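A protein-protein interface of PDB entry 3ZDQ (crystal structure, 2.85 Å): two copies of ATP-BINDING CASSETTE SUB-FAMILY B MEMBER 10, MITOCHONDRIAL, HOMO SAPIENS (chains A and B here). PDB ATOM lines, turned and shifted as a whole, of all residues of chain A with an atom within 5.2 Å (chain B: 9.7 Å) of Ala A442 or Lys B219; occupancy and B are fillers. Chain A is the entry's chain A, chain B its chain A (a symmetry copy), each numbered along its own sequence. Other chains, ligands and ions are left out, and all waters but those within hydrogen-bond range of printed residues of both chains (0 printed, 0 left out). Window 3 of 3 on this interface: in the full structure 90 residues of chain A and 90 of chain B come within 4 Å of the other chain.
No position is printed for both chains.
Of the 8 pairs that touch across the chains among the printed residues, none has its exchanged pair printed and touching as well.
Tyr A440 touches Val B214 (OH to CG2, 3.6 Å).
Tyr A440 touches Phe B217 (O to CD1, 3.9 Å).
CD of Pro A445 touches CE of Lys B219, 3.7 Å away.
Lys A500 touches Ala B216.
Phe B217 touches Lys A500 (CA to NZ, 3.9 Å).
The guanidinium group (NE) of Arg B207 is in salt-bridge range of the side-chain carboxylate (OE2) of Glu B223 (3.0 Å).
The backbone NH (N) of Lys B219 lies within hydrogen-bond range of the backbone carbonyl oxygen (O) of Val B214.
The side-chain amino group of Lys B219 sits at hydrogen-bond distance from the backbone carbonyl oxygen of Phe B217, at 2.8 Å.
The side-chain carboxylate (OE1) of Glu B223 lies within salt-bridge range of the side-chain amino group (NZ) of Lys B226 (2.9 Å).
Of the printed residues of chain B, Lys A500 touches Ala B216 (3.6 Å) and Phe B217 (3.9 Å).
Of the printed residues of chain A, Val B214 touches Tyr A440 (3.6 Å).
Of the printed residues of chain A, Phe B217 touches Tyr A440 and Lys A500.
Of the printed residues of chain A, Lys B219 touches Tyr A440 (2.9 Å), Ala A442 (2.9 Å) and Pro A445 (3.7 Å).
Printed residues of chain A within 4 Å of Glu B223: Tyr A440.
The nearest printed residue of chain A that does not touch Lys B219 is Asp A443 (4.3 Å).
The nearest printed residue of chain A that does not touch Ala B216 is Tyr A440 (6.8 Å).
Of the 11 printed residues of chain A, 4 touch a printed residue of chain B.
Hydrophobic or aromatic side chains of chain A within 4 Å of the printed part of chain B: Tyr A440 and Pro A445.
Along chain A the printed residues that touch a printed residue of chain B span positions 440 to 500.
Of the 20 printed residues of chain B, 5 touch a printed residue of chain A.
O of Tyr A440 is in hydrogen-bond range of NZ of Lys B219 (2.9 Å).
OH of Tyr A440 lies within hydrogen-bond range of OE2 of Glu B223 (2.7 Å).
The side-chain amino group (NZ) of Lys B219 sits at hydrogen-bond distance from the backbone carbonyl oxygen (O) of Ala A442 (2.9 Å).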
ATOM      1  N   ILE A 438      33.429  16.239  19.983  1.00  0.00           N
ATOM      2  CA  ILE A 438      34.684  16.525  19.277  1.00  0.00           C
ATOM      3  C   ILE A 438      35.208  15.232  18.595  1.00  0.00           C
ATOM      4  O   ILE A 438      35.555  15.280  17.412  1.00  0.00           O
ATOM      5  CB  ILE A 438      35.744  17.161  20.228  1.00  0.00           C
ATOM      6  CG1 ILE A 438      35.275  18.548  20.726  1.00  0.00           C
ATOM      7  CG2 ILE A 438      37.142  17.253  19.566  1.00  0.00           C
ATOM      8  CD1 ILE A 438      36.121  19.149  21.926  1.00  0.00           C
ATOM      9  N   ALA A 439      35.220  14.090  19.338  1.00  0.00           N
ATOM     10  CA  ALA A 439      35.690  12.762  18.902  1.00  0.00           C
ATOM     11  C   ALA A 439      34.987  12.256  17.628  1.00  0.00           C
ATOM     12  O   ALA A 439      35.579  11.505  16.853  1.00  0.00           O
ATOM     13  CB  ALA A 439      35.493  11.760  20.015  1.00  0.00           C
ATOM     14  N   TYR A 440      33.731  12.692  17.416  1.00  0.00           N
ATOM     15  CA  TYR A 440      32.854  12.376  16.289  1.00  0.00           C
ATOM     16  C   TYR A 440      33.506  12.659  14.922  1.00  0.00           C
ATOM     17  O   TYR A 440      33.106  12.026  13.931  1.00  0.00           O
ATOM     18  CB  TYR A 440      31.567  13.195  16.420  1.00  0.00           C
ATOM     19  CG  TYR A 440      30.335  12.544  15.839  1.00  0.00           C
ATOM     20  CD1 TYR A 440      29.821  11.369  16.379  1.00  0.00           C
ATOM     21  CD2 TYR A 440      29.634  13.141  14.796  1.00  0.00           C
ATOM     22  CE1 TYR A 440      28.670  10.778  15.863  1.00  0.00           C
ATOM     23  CE2 TYR A 440      28.461  12.576  14.293  1.00  0.00           C
ATOM     24  CZ  TYR A 440      27.977  11.400  14.839  1.00  0.00           C
ATOM     25  OH  TYR A 440      26.831  10.837  14.335  1.00  0.00           O
ATOM     26  N   GLY A 441      34.472  13.603  14.885  1.00  0.00           N
ATOM     27  CA  GLY A 441      35.220  13.976  13.691  1.00  0.00           C
ATOM     28  C   GLY A 441      36.084  12.835  13.175  1.00  0.00           C
ATOM     29  O   GLY A 441      36.195  12.633  11.959  1.00  0.00           O
ATOM     30  N   ALA A 442      36.665  12.043  14.097  1.00  0.00           N
ATOM     31  CA  ALA A 442      37.527  10.904  13.787  1.00  0.00           C
ATOM     32  C   ALA A 442      36.778   9.744  13.127  1.00  0.00           C
ATOM     33  O   ALA A 442      35.626   9.486  13.477  1.00  0.00           O
ATOM     34  CB  ALA A 442      38.181  10.403  15.061  1.00  0.00           C
ATOM     35  N   ASP A 443      37.461   8.987  12.233  1.00  0.00           N
ATOM     36  CA  ASP A 443      36.898   7.785  11.596  1.00  0.00           C
ATOM     37  C   ASP A 443      36.529   6.743  12.664  1.00  0.00           C
ATOM     38  O   ASP A 443      35.568   5.988  12.483  1.00  0.00           O
ATOM     39  CB  ASP A 443      37.881   7.180  10.574  1.00  0.00           C
ATOM     40  CG  ASP A 443      37.933   7.855   9.200  1.00  0.00           C
ATOM     41  OD1 ASP A 443      37.169   8.836   8.979  1.00  0.00           O
ATOM     42  OD2 ASP A 443      38.727   7.395   8.342  1.00  0.00           O
ATOM     43  N   ASP A 444      37.276   6.755  13.801  1.00  0.00           N
ATOM     44  CA  ASP A 444      37.104   5.888  14.971  1.00  0.00           C
ATOM     45  C   ASP A 444      37.049   6.750  16.252  1.00  0.00           C
ATOM     46  O   ASP A 444      38.074   6.899  16.931  1.00  0.00           O
ATOM     47  CB  ASP A 444      38.242   4.850  15.041  1.00  0.00           C
ATOM     48  CG  ASP A 444      37.922   3.601  15.846  1.00  0.00           C
ATOM     49  OD1 ASP A 444      37.350   3.733  16.960  1.00  0.00           O
ATOM     50  OD2 ASP A 444      38.307   2.493  15.399  1.00  0.00           O
ATOM     51  N   PRO A 445      35.855   7.311  16.597  1.00  0.00           N
ATOM     52  CA  PRO A 445      35.759   8.191  17.781  1.00  0.00           C
ATOM     53  C   PRO A 445      36.078   7.534  19.138  1.00  0.00           C
ATOM     54  O   PRO A 445      36.360   8.262  20.094  1.00  0.00           O
ATOM     55  CB  PRO A 445      34.312   8.701  17.751  1.00  0.00           C
ATOM     56  CG  PRO A 445      33.604   7.881  16.777  1.00  0.00           C
ATOM     57  CD  PRO A 445      34.579   7.265  15.852  1.00  0.00           C
ATOM     58  N   VAL A 448      40.117   7.763  19.740  1.00  0.00           N
ATOM     59  CA  VAL A 448      40.822   9.031  19.991  1.00  0.00           C
ATOM     60  C   VAL A 448      41.218   9.130  21.457  1.00  0.00           C
ATOM     61  O   VAL A 448      40.476   8.713  22.355  1.00  0.00           O
ATOM     62  CB  VAL A 448      40.147  10.347  19.514  1.00  0.00           C
ATOM     63  CG1 VAL A 448      40.047  10.408  18.002  1.00  0.00           C
ATOM     64  CG2 VAL A 448      38.798  10.578  20.159  1.00  0.00           C
ATOM     65  N   LEU A 499      39.836  17.557  13.838  1.00  0.00           N
ATOM     66  CA  LEU A 499      40.055  16.148  14.161  1.00  0.00           C
ATOM     67  C   LEU A 499      39.771  15.278  12.948  1.00  0.00           C
ATOM     68  O   LEU A 499      40.504  14.316  12.719  1.00  0.00           O
ATOM     69  CB  LEU A 499      39.223  15.689  15.360  1.00  0.00           C
ATOM     70  CG  LEU A 499      39.603  14.317  15.942  1.00  0.00           C
ATOM     71  CD1 LEU A 499      40.904  14.375  16.750  1.00  0.00           C
ATOM     72  CD2 LEU A 499      38.499  13.785  16.794  1.00  0.00           C
ATOM     73  N   LYS A 500      38.739  15.635  12.147  1.00  0.00           N
ATOM     74  CA  LYS A 500      38.419  14.922  10.901  1.00  0.00           C
ATOM     75  C   LYS A 500      39.612  15.074   9.934  1.00  0.00           C
ATOM     76  O   LYS A 500      40.050  14.085   9.340  1.00  0.00           O
ATOM     77  CB  LYS A 500      37.101  15.450  10.263  1.00  0.00           C
ATOM     78  CG  LYS A 500      36.543  14.550   9.160  1.00  0.00           C
ATOM     79  CD  LYS A 500      35.735  15.302   8.111  1.00  0.00           C
ATOM     80  CE  LYS A 500      34.258  14.969   8.078  1.00  0.00           C
ATOM     81  NZ  LYS A 500      34.004  13.529   7.800  1.00  0.00           N
ATOM     82  N   LEU B 203      18.268   8.497  22.062  1.00  0.00           N
ATOM     83  CA  LEU B 203      19.437   8.396  21.187  1.00  0.00           C
ATOM     84  C   LEU B 203      18.970   8.177  19.731  1.00  0.00           C
ATOM     85  O   LEU B 203      19.376   8.918  18.841  1.00  0.00           O
ATOM     86  CB  LEU B 203      20.340   7.229  21.664  1.00  0.00           C
ATOM     87  CG  LEU B 203      21.461   6.774  20.741  1.00  0.00           C
ATOM     88  CD1 LEU B 203      22.608   7.692  20.823  1.00  0.00           C
ATOM     89  CD2 LEU B 203      21.945   5.413  21.116  1.00  0.00           C
ATOM     90  N   ARG B 207      19.415  10.902  16.599  1.00  0.00           N
ATOM     91  CA  ARG B 207      20.192  10.452  15.446  1.00  0.00           C
ATOM     92  C   ARG B 207      19.364  10.353  14.167  1.00  0.00           C
ATOM     93  O   ARG B 207      19.914  10.587  13.106  1.00  0.00           O
ATOM     94  CB  ARG B 207      20.852   9.116  15.755  1.00  0.00           C
ATOM     95  CG  ARG B 207      22.236   9.264  16.333  1.00  0.00           C
ATOM     96  CD  ARG B 207      22.305   9.857  17.725  1.00  0.00           C
ATOM     97  NE  ARG B 207      23.687  10.082  18.142  1.00  0.00           N
ATOM     98  CZ  ARG B 207      24.034  10.641  19.291  1.00  0.00           C
ATOM     99  NH1 ARG B 207      23.103  11.030  20.152  1.00  0.00           N
ATOM    100  NH2 ARG B 207      25.308  10.815  19.593  1.00  0.00           N
ATOM    101  N   ASN B 210      18.700  13.923  13.142  1.00  0.00           N
ATOM    102  CA  ASN B 210      19.925  14.595  12.695  1.00  0.00           C
ATOM    103  C   ASN B 210      20.737  13.681  11.805  1.00  0.00           C
ATOM    104  O   ASN B 210      21.972  13.673  11.879  1.00  0.00           O
ATOM    105  CB  ASN B 210      20.752  15.036  13.902  1.00  0.00           C
ATOM    106  CG  ASN B 210      20.048  16.056  14.747  1.00  0.00           C
ATOM    107  OD1 ASN B 210      19.908  17.226  14.374  1.00  0.00           O
ATOM    108  ND2 ASN B 210      19.528  15.610  15.874  1.00  0.00           N
ATOM    109  N   VAL B 211      20.041  12.940  10.930  1.00  0.00           N
ATOM    110  CA  VAL B 211      20.609  11.959  10.023  1.00  0.00           C
ATOM    111  C   VAL B 211      21.591  12.651   9.074  1.00  0.00           C
ATOM    112  O   VAL B 211      22.610  12.048   8.742  1.00  0.00           O
ATOM    113  CB  VAL B 211      19.480  11.148   9.309  1.00  0.00           C
ATOM    114  CG1 VAL B 211      18.673  11.986   8.316  1.00  0.00           C
ATOM    115  CG2 VAL B 211      19.992   9.850   8.685  1.00  0.00           C
ATOM    116  N   ARG B 212      21.329  13.932   8.702  1.00  0.00           N
ATOM    117  CA  ARG B 212      22.192  14.749   7.835  1.00  0.00           C
ATOM    118  C   ARG B 212      23.581  14.922   8.482  1.00  0.00           C
ATOM    119  O   ARG B 212      24.563  14.687   7.797  1.00  0.00           O
ATOM    120  CB  ARG B 212      21.535  16.111   7.526  1.00  0.00           C
ATOM    121  CG  ARG B 212      20.484  16.013   6.428  1.00  0.00           C
ATOM    122  CD  ARG B 212      19.466  17.145   6.436  1.00  0.00           C
ATOM    123  NE  ARG B 212      18.125  16.694   6.012  1.00  0.00           N
ATOM    124  CZ  ARG B 212      17.227  16.128   6.823  1.00  0.00           C
ATOM    125  NH1 ARG B 212      17.506  15.937   8.113  1.00  0.00           N
ATOM    126  NH2 ARG B 212      16.046  15.738   6.348  1.00  0.00           N
ATOM    127  N   THR B 213      23.665  15.228   9.809  1.00  0.00           N
ATOM    128  CA  THR B 213      24.924  15.346  10.584  1.00  0.00           C
ATOM    129  C   THR B 213      25.598  13.960  10.711  1.00  0.00           C
ATOM    130  O   THR B 213      26.811  13.872  10.566  1.00  0.00           O
ATOM    131  CB  THR B 213      24.641  15.948  11.989  1.00  0.00           C
ATOM    132  OG1 THR B 213      23.938  17.185  11.865  1.00  0.00           O
ATOM    133  CG2 THR B 213      25.906  16.149  12.827  1.00  0.00           C
ATOM    134  N   VAL B 214      24.813  12.894  11.001  1.00  0.00           N
ATOM    135  CA  VAL B 214      25.281  11.510  11.116  1.00  0.00           C
ATOM    136  C   VAL B 214      25.963  11.115   9.776  1.00  0.00           C
ATOM    137  O   VAL B 214      27.154  10.782   9.821  1.00  0.00           O
ATOM    138  CB  VAL B 214      24.123  10.547  11.523  1.00  0.00           C
ATOM    139  CG1 VAL B 214      24.554   9.080  11.460  1.00  0.00           C
ATOM    140  CG2 VAL B 214      23.564  10.888  12.909  1.00  0.00           C
ATOM    141  N   ARG B 215      25.245  11.226   8.596  1.00  0.00           N
ATOM    142  CA  ARG B 215      25.770  10.972   7.247  1.00  0.00           C
ATOM    143  C   ARG B 215      27.076  11.674   7.006  1.00  0.00           C
ATOM    144  O   ARG B 215      28.051  11.049   6.565  1.00  0.00           O
ATOM    145  CB  ARG B 215      24.834  11.529   6.179  1.00  0.00           C
ATOM    146  CG  ARG B 215      23.616  10.757   5.890  1.00  0.00           C
ATOM    147  CD  ARG B 215      23.625  10.087   4.536  1.00  0.00           C
ATOM    148  NE  ARG B 215      23.163   8.719   4.760  1.00  0.00           N
ATOM    149  CZ  ARG B 215      21.893   8.355   4.859  1.00  0.00           C
ATOM    150  NH1 ARG B 215      20.924   9.225   4.611  1.00  0.00           N
ATOM    151  NH2 ARG B 215      21.578   7.106   5.159  1.00  0.00           N
ATOM    152  N   ALA B 216      27.055  13.026   7.222  1.00  0.00           N
ATOM    153  CA  ALA B 216      28.145  13.979   7.002  1.00  0.00           C
ATOM    154  C   ALA B 216      29.454  13.518   7.587  1.00  0.00           C
ATOM    155  O   ALA B 216      30.493  13.837   7.016  1.00  0.00           O
ATOM    156  CB  ALA B 216      27.787  15.335   7.584  1.00  0.00           C
ATOM    157  N   PHE B 217      29.419  12.786   8.711  1.00  0.00           N
ATOM    158  CA  PHE B 217      30.619  12.299   9.374  1.00  0.00           C
ATOM    159  C   PHE B 217      30.817  10.788   9.202  1.00  0.00           C
ATOM    160  O   PHE B 217      31.679  10.223   9.881  1.00  0.00           O
ATOM    161  CB  PHE B 217      30.548  12.644  10.869  1.00  0.00           C
ATOM    162  CG  PHE B 217      30.693  14.116  11.152  1.00  0.00           C
ATOM    163  CD1 PHE B 217      31.947  14.680  11.349  1.00  0.00           C
ATOM    164  CD2 PHE B 217      29.583  14.939  11.217  1.00  0.00           C
ATOM    165  CE1 PHE B 217      32.084  16.043  11.596  1.00  0.00           C
ATOM    166  CE2 PHE B 217      29.725  16.303  11.447  1.00  0.00           C
ATOM    167  CZ  PHE B 217      30.977  16.844  11.630  1.00  0.00           C
ATOM    168  N   GLY B 218      30.029  10.153   8.326  1.00  0.00           N
ATOM    169  CA  GLY B 218      30.074   8.717   8.072  1.00  0.00           C
ATOM    170  C   GLY B 218      29.896   7.888   9.332  1.00  0.00           C
ATOM    171  O   GLY B 218      30.645   6.931   9.554  1.00  0.00           O
ATOM    172  N   LYS B 219      28.905   8.259  10.171  1.00  0.00           N
ATOM    173  CA  LYS B 219      28.679   7.623  11.465  1.00  0.00           C
ATOM    174  C   LYS B 219      27.403   6.793  11.548  1.00  0.00           C
ATOM    175  O   LYS B 219      27.035   6.363  12.638  1.00  0.00           O
ATOM    176  CB  LYS B 219      28.688   8.684  12.564  1.00  0.00           C
ATOM    177  CG  LYS B 219      30.049   9.355  12.765  1.00  0.00           C
ATOM    178  CD  LYS B 219      31.137   8.345  13.153  1.00  0.00           C
ATOM    179  CE  LYS B 219      32.441   9.016  13.457  1.00  0.00           C
ATOM    180  NZ  LYS B 219      33.042   9.651  12.262  1.00  0.00           N
ATOM    181  N   GLU B 220      26.768   6.493  10.408  1.00  0.00           N
ATOM    182  CA  GLU B 220      25.565   5.661  10.398  1.00  0.00           C
ATOM    183  C   GLU B 220      25.872   4.303  11.007  1.00  0.00           C
ATOM    184  O   GLU B 220      25.155   3.898  11.909  1.00  0.00           O
ATOM    185  CB  GLU B 220      24.969   5.498   8.985  1.00  0.00           C
ATOM    186  CG  GLU B 220      24.733   6.792   8.209  1.00  0.00           C
ATOM    187  CD  GLU B 220      25.728   7.043   7.091  1.00  0.00           C
ATOM    188  OE1 GLU B 220      26.944   7.133   7.384  1.00  0.00           O
ATOM    189  OE2 GLU B 220      25.297   7.123   5.917  1.00  0.00           O
ATOM    190  N   MET B 221      26.974   3.635  10.576  1.00  0.00           N
ATOM    191  CA  MET B 221      27.375   2.317  11.083  1.00  0.00           C
ATOM    192  C   MET B 221      27.684   2.328  12.597  1.00  0.00           C
ATOM    193  O   MET B 221      27.332   1.373  13.301  1.00  0.00           O
ATOM    194  CB  MET B 221      28.563   1.752  10.304  1.00  0.00           C
ATOM    195  CG  MET B 221      28.178   1.007   9.030  1.00  0.00           C
ATOM    196  SD  MET B 221      26.673  -0.042   9.090  1.00  0.00           S
ATOM    197  CE  MET B 221      27.085  -1.276  10.491  1.00  0.00           C
ATOM    198  N   THR B 222      28.308   3.428  13.082  1.00  0.00           N
ATOM    199  CA  THR B 222      28.672   3.685  14.476  1.00  0.00           C
ATOM    200  C   THR B 222      27.405   3.826  15.323  1.00  0.00           C
ATOM    201  O   THR B 222      27.309   3.209  16.391  1.00  0.00           O
ATOM    202  CB  THR B 222      29.552   4.945  14.537  1.00  0.00           C
ATOM    203  OG1 THR B 222      30.758   4.717  13.788  1.00  0.00           O
ATOM    204  CG2 THR B 222      29.876   5.385  15.968  1.00  0.00           C
ATOM    205  N   GLU B 223      26.432   4.625  14.845  1.00  0.00           N
ATOM    206  CA  GLU B 223      25.182   4.856  15.555  1.00  0.00           C
ATOM    207  C   GLU B 223      24.368   3.558  15.656  1.00  0.00           C
ATOM    208  O   GLU B 223      23.842   3.270  16.731  1.00  0.00           O
ATOM    209  CB  GLU B 223      24.365   5.997  14.904  1.00  0.00           C
ATOM    210  CG  GLU B 223      25.021   7.386  14.946  1.00  0.00           C
ATOM    211  CD  GLU B 223      25.475   8.008  16.264  1.00  0.00           C
ATOM    212  OE1 GLU B 223      25.476   7.328  17.315  1.00  0.00           O
ATOM    213  OE2 GLU B 223      25.847   9.202  16.231  1.00  0.00           O
ATOM    214  N   ILE B 224      24.335   2.752  14.564  1.00  0.00           N
ATOM    215  CA  ILE B 224      23.665   1.446  14.489  1.00  0.00           C
ATOM    216  C   ILE B 224      24.259   0.516  15.566  1.00  0.00           C
ATOM    217  O   ILE B 224      23.501  -0.100  16.313  1.00  0.00           O
ATOM    218  CB  ILE B 224      23.754   0.841  13.047  1.00  0.00           C
ATOM    219  CG1 ILE B 224      22.847   1.644  12.047  1.00  0.00           C
ATOM    220  CG2 ILE B 224      23.411  -0.649  13.046  1.00  0.00           C
ATOM    221  CD1 ILE B 224      23.225   1.615  10.551  1.00  0.00           C
ATOM    222  N   GLU B 225      25.595   0.473  15.689  1.00  0.00           N
ATOM    223  CA  GLU B 225      26.278  -0.376  16.668  1.00  0.00           C
ATOM    224  C   GLU B 225      26.087   0.163  18.073  1.00  0.00           C
ATOM    225  O   GLU B 225      25.969  -0.637  18.998  1.00  0.00           O
ATOM    226  CB  GLU B 225      27.772  -0.528  16.341  1.00  0.00           C
ATOM    227  CG  GLU B 225      28.029  -1.355  15.092  1.00  0.00           C
ATOM    228  CD  GLU B 225      29.437  -1.301  14.528  1.00  0.00           C
ATOM    229  OE1 GLU B 225      30.390  -1.634  15.270  1.00  0.00           O
ATOM    230  OE2 GLU B 225      29.580  -0.999  13.320  1.00  0.00           O
ATOM    231  N   LYS B 226      26.032   1.504  18.236  1.00  0.00           N
ATOM    232  CA  LYS B 226      25.814   2.161  19.537  1.00  0.00           C
ATOM    233  C   LYS B 226      24.456   1.789  20.085  1.00  0.00           C
ATOM    234  O   LYS B 226      24.368   1.357  21.226  1.00  0.00           O
ATOM    235  CB  LYS B 226      25.921   3.692  19.416  1.00  0.00           C
ATOM    236  CG  LYS B 226      26.110   4.421  20.755  1.00  0.00           C
ATOM    237  CD  LYS B 226      26.016   5.952  20.614  1.00  0.00           C
ATOM    238  CE  LYS B 226      27.242   6.603  20.017  1.00  0.00           C
ATOM    239  NZ  LYS B 226      26.988   8.022  19.651  1.00  0.00           N
ATOM    240  N   TYR B 227      23.404   1.943  19.255  1.00  0.00           N
ATOM    241  CA  TYR B 227      22.010   1.647  19.569  1.00  0.00           C
ATOM    242  C   TYR B 227      21.854   0.162  19.899  1.00  0.00           C
ATOM    243  O   TYR B 227      21.261  -0.165  20.931  1.00  0.00           O
ATOM    244  CB  TYR B 227      21.098   2.063  18.404  1.00  0.00           C
ATOM    245  CG  TYR B 227      19.636   1.790  18.662  1.00  0.00           C
ATOM    246  CD1 TYR B 227      18.897   2.596  19.530  1.00  0.00           C
ATOM    247  CD2 TYR B 227      18.994   0.704  18.070  1.00  0.00           C
ATOM    248  CE1 TYR B 227      17.550   2.343  19.781  1.00  0.00           C
ATOM    249  CE2 TYR B 227      17.650   0.440  18.316  1.00  0.00           C
ATOM    250  CZ  TYR B 227      16.927   1.271  19.159  1.00  0.00           C
ATOM    251  OH  TYR B 227      15.594   1.014  19.398  1.00  0.00           O
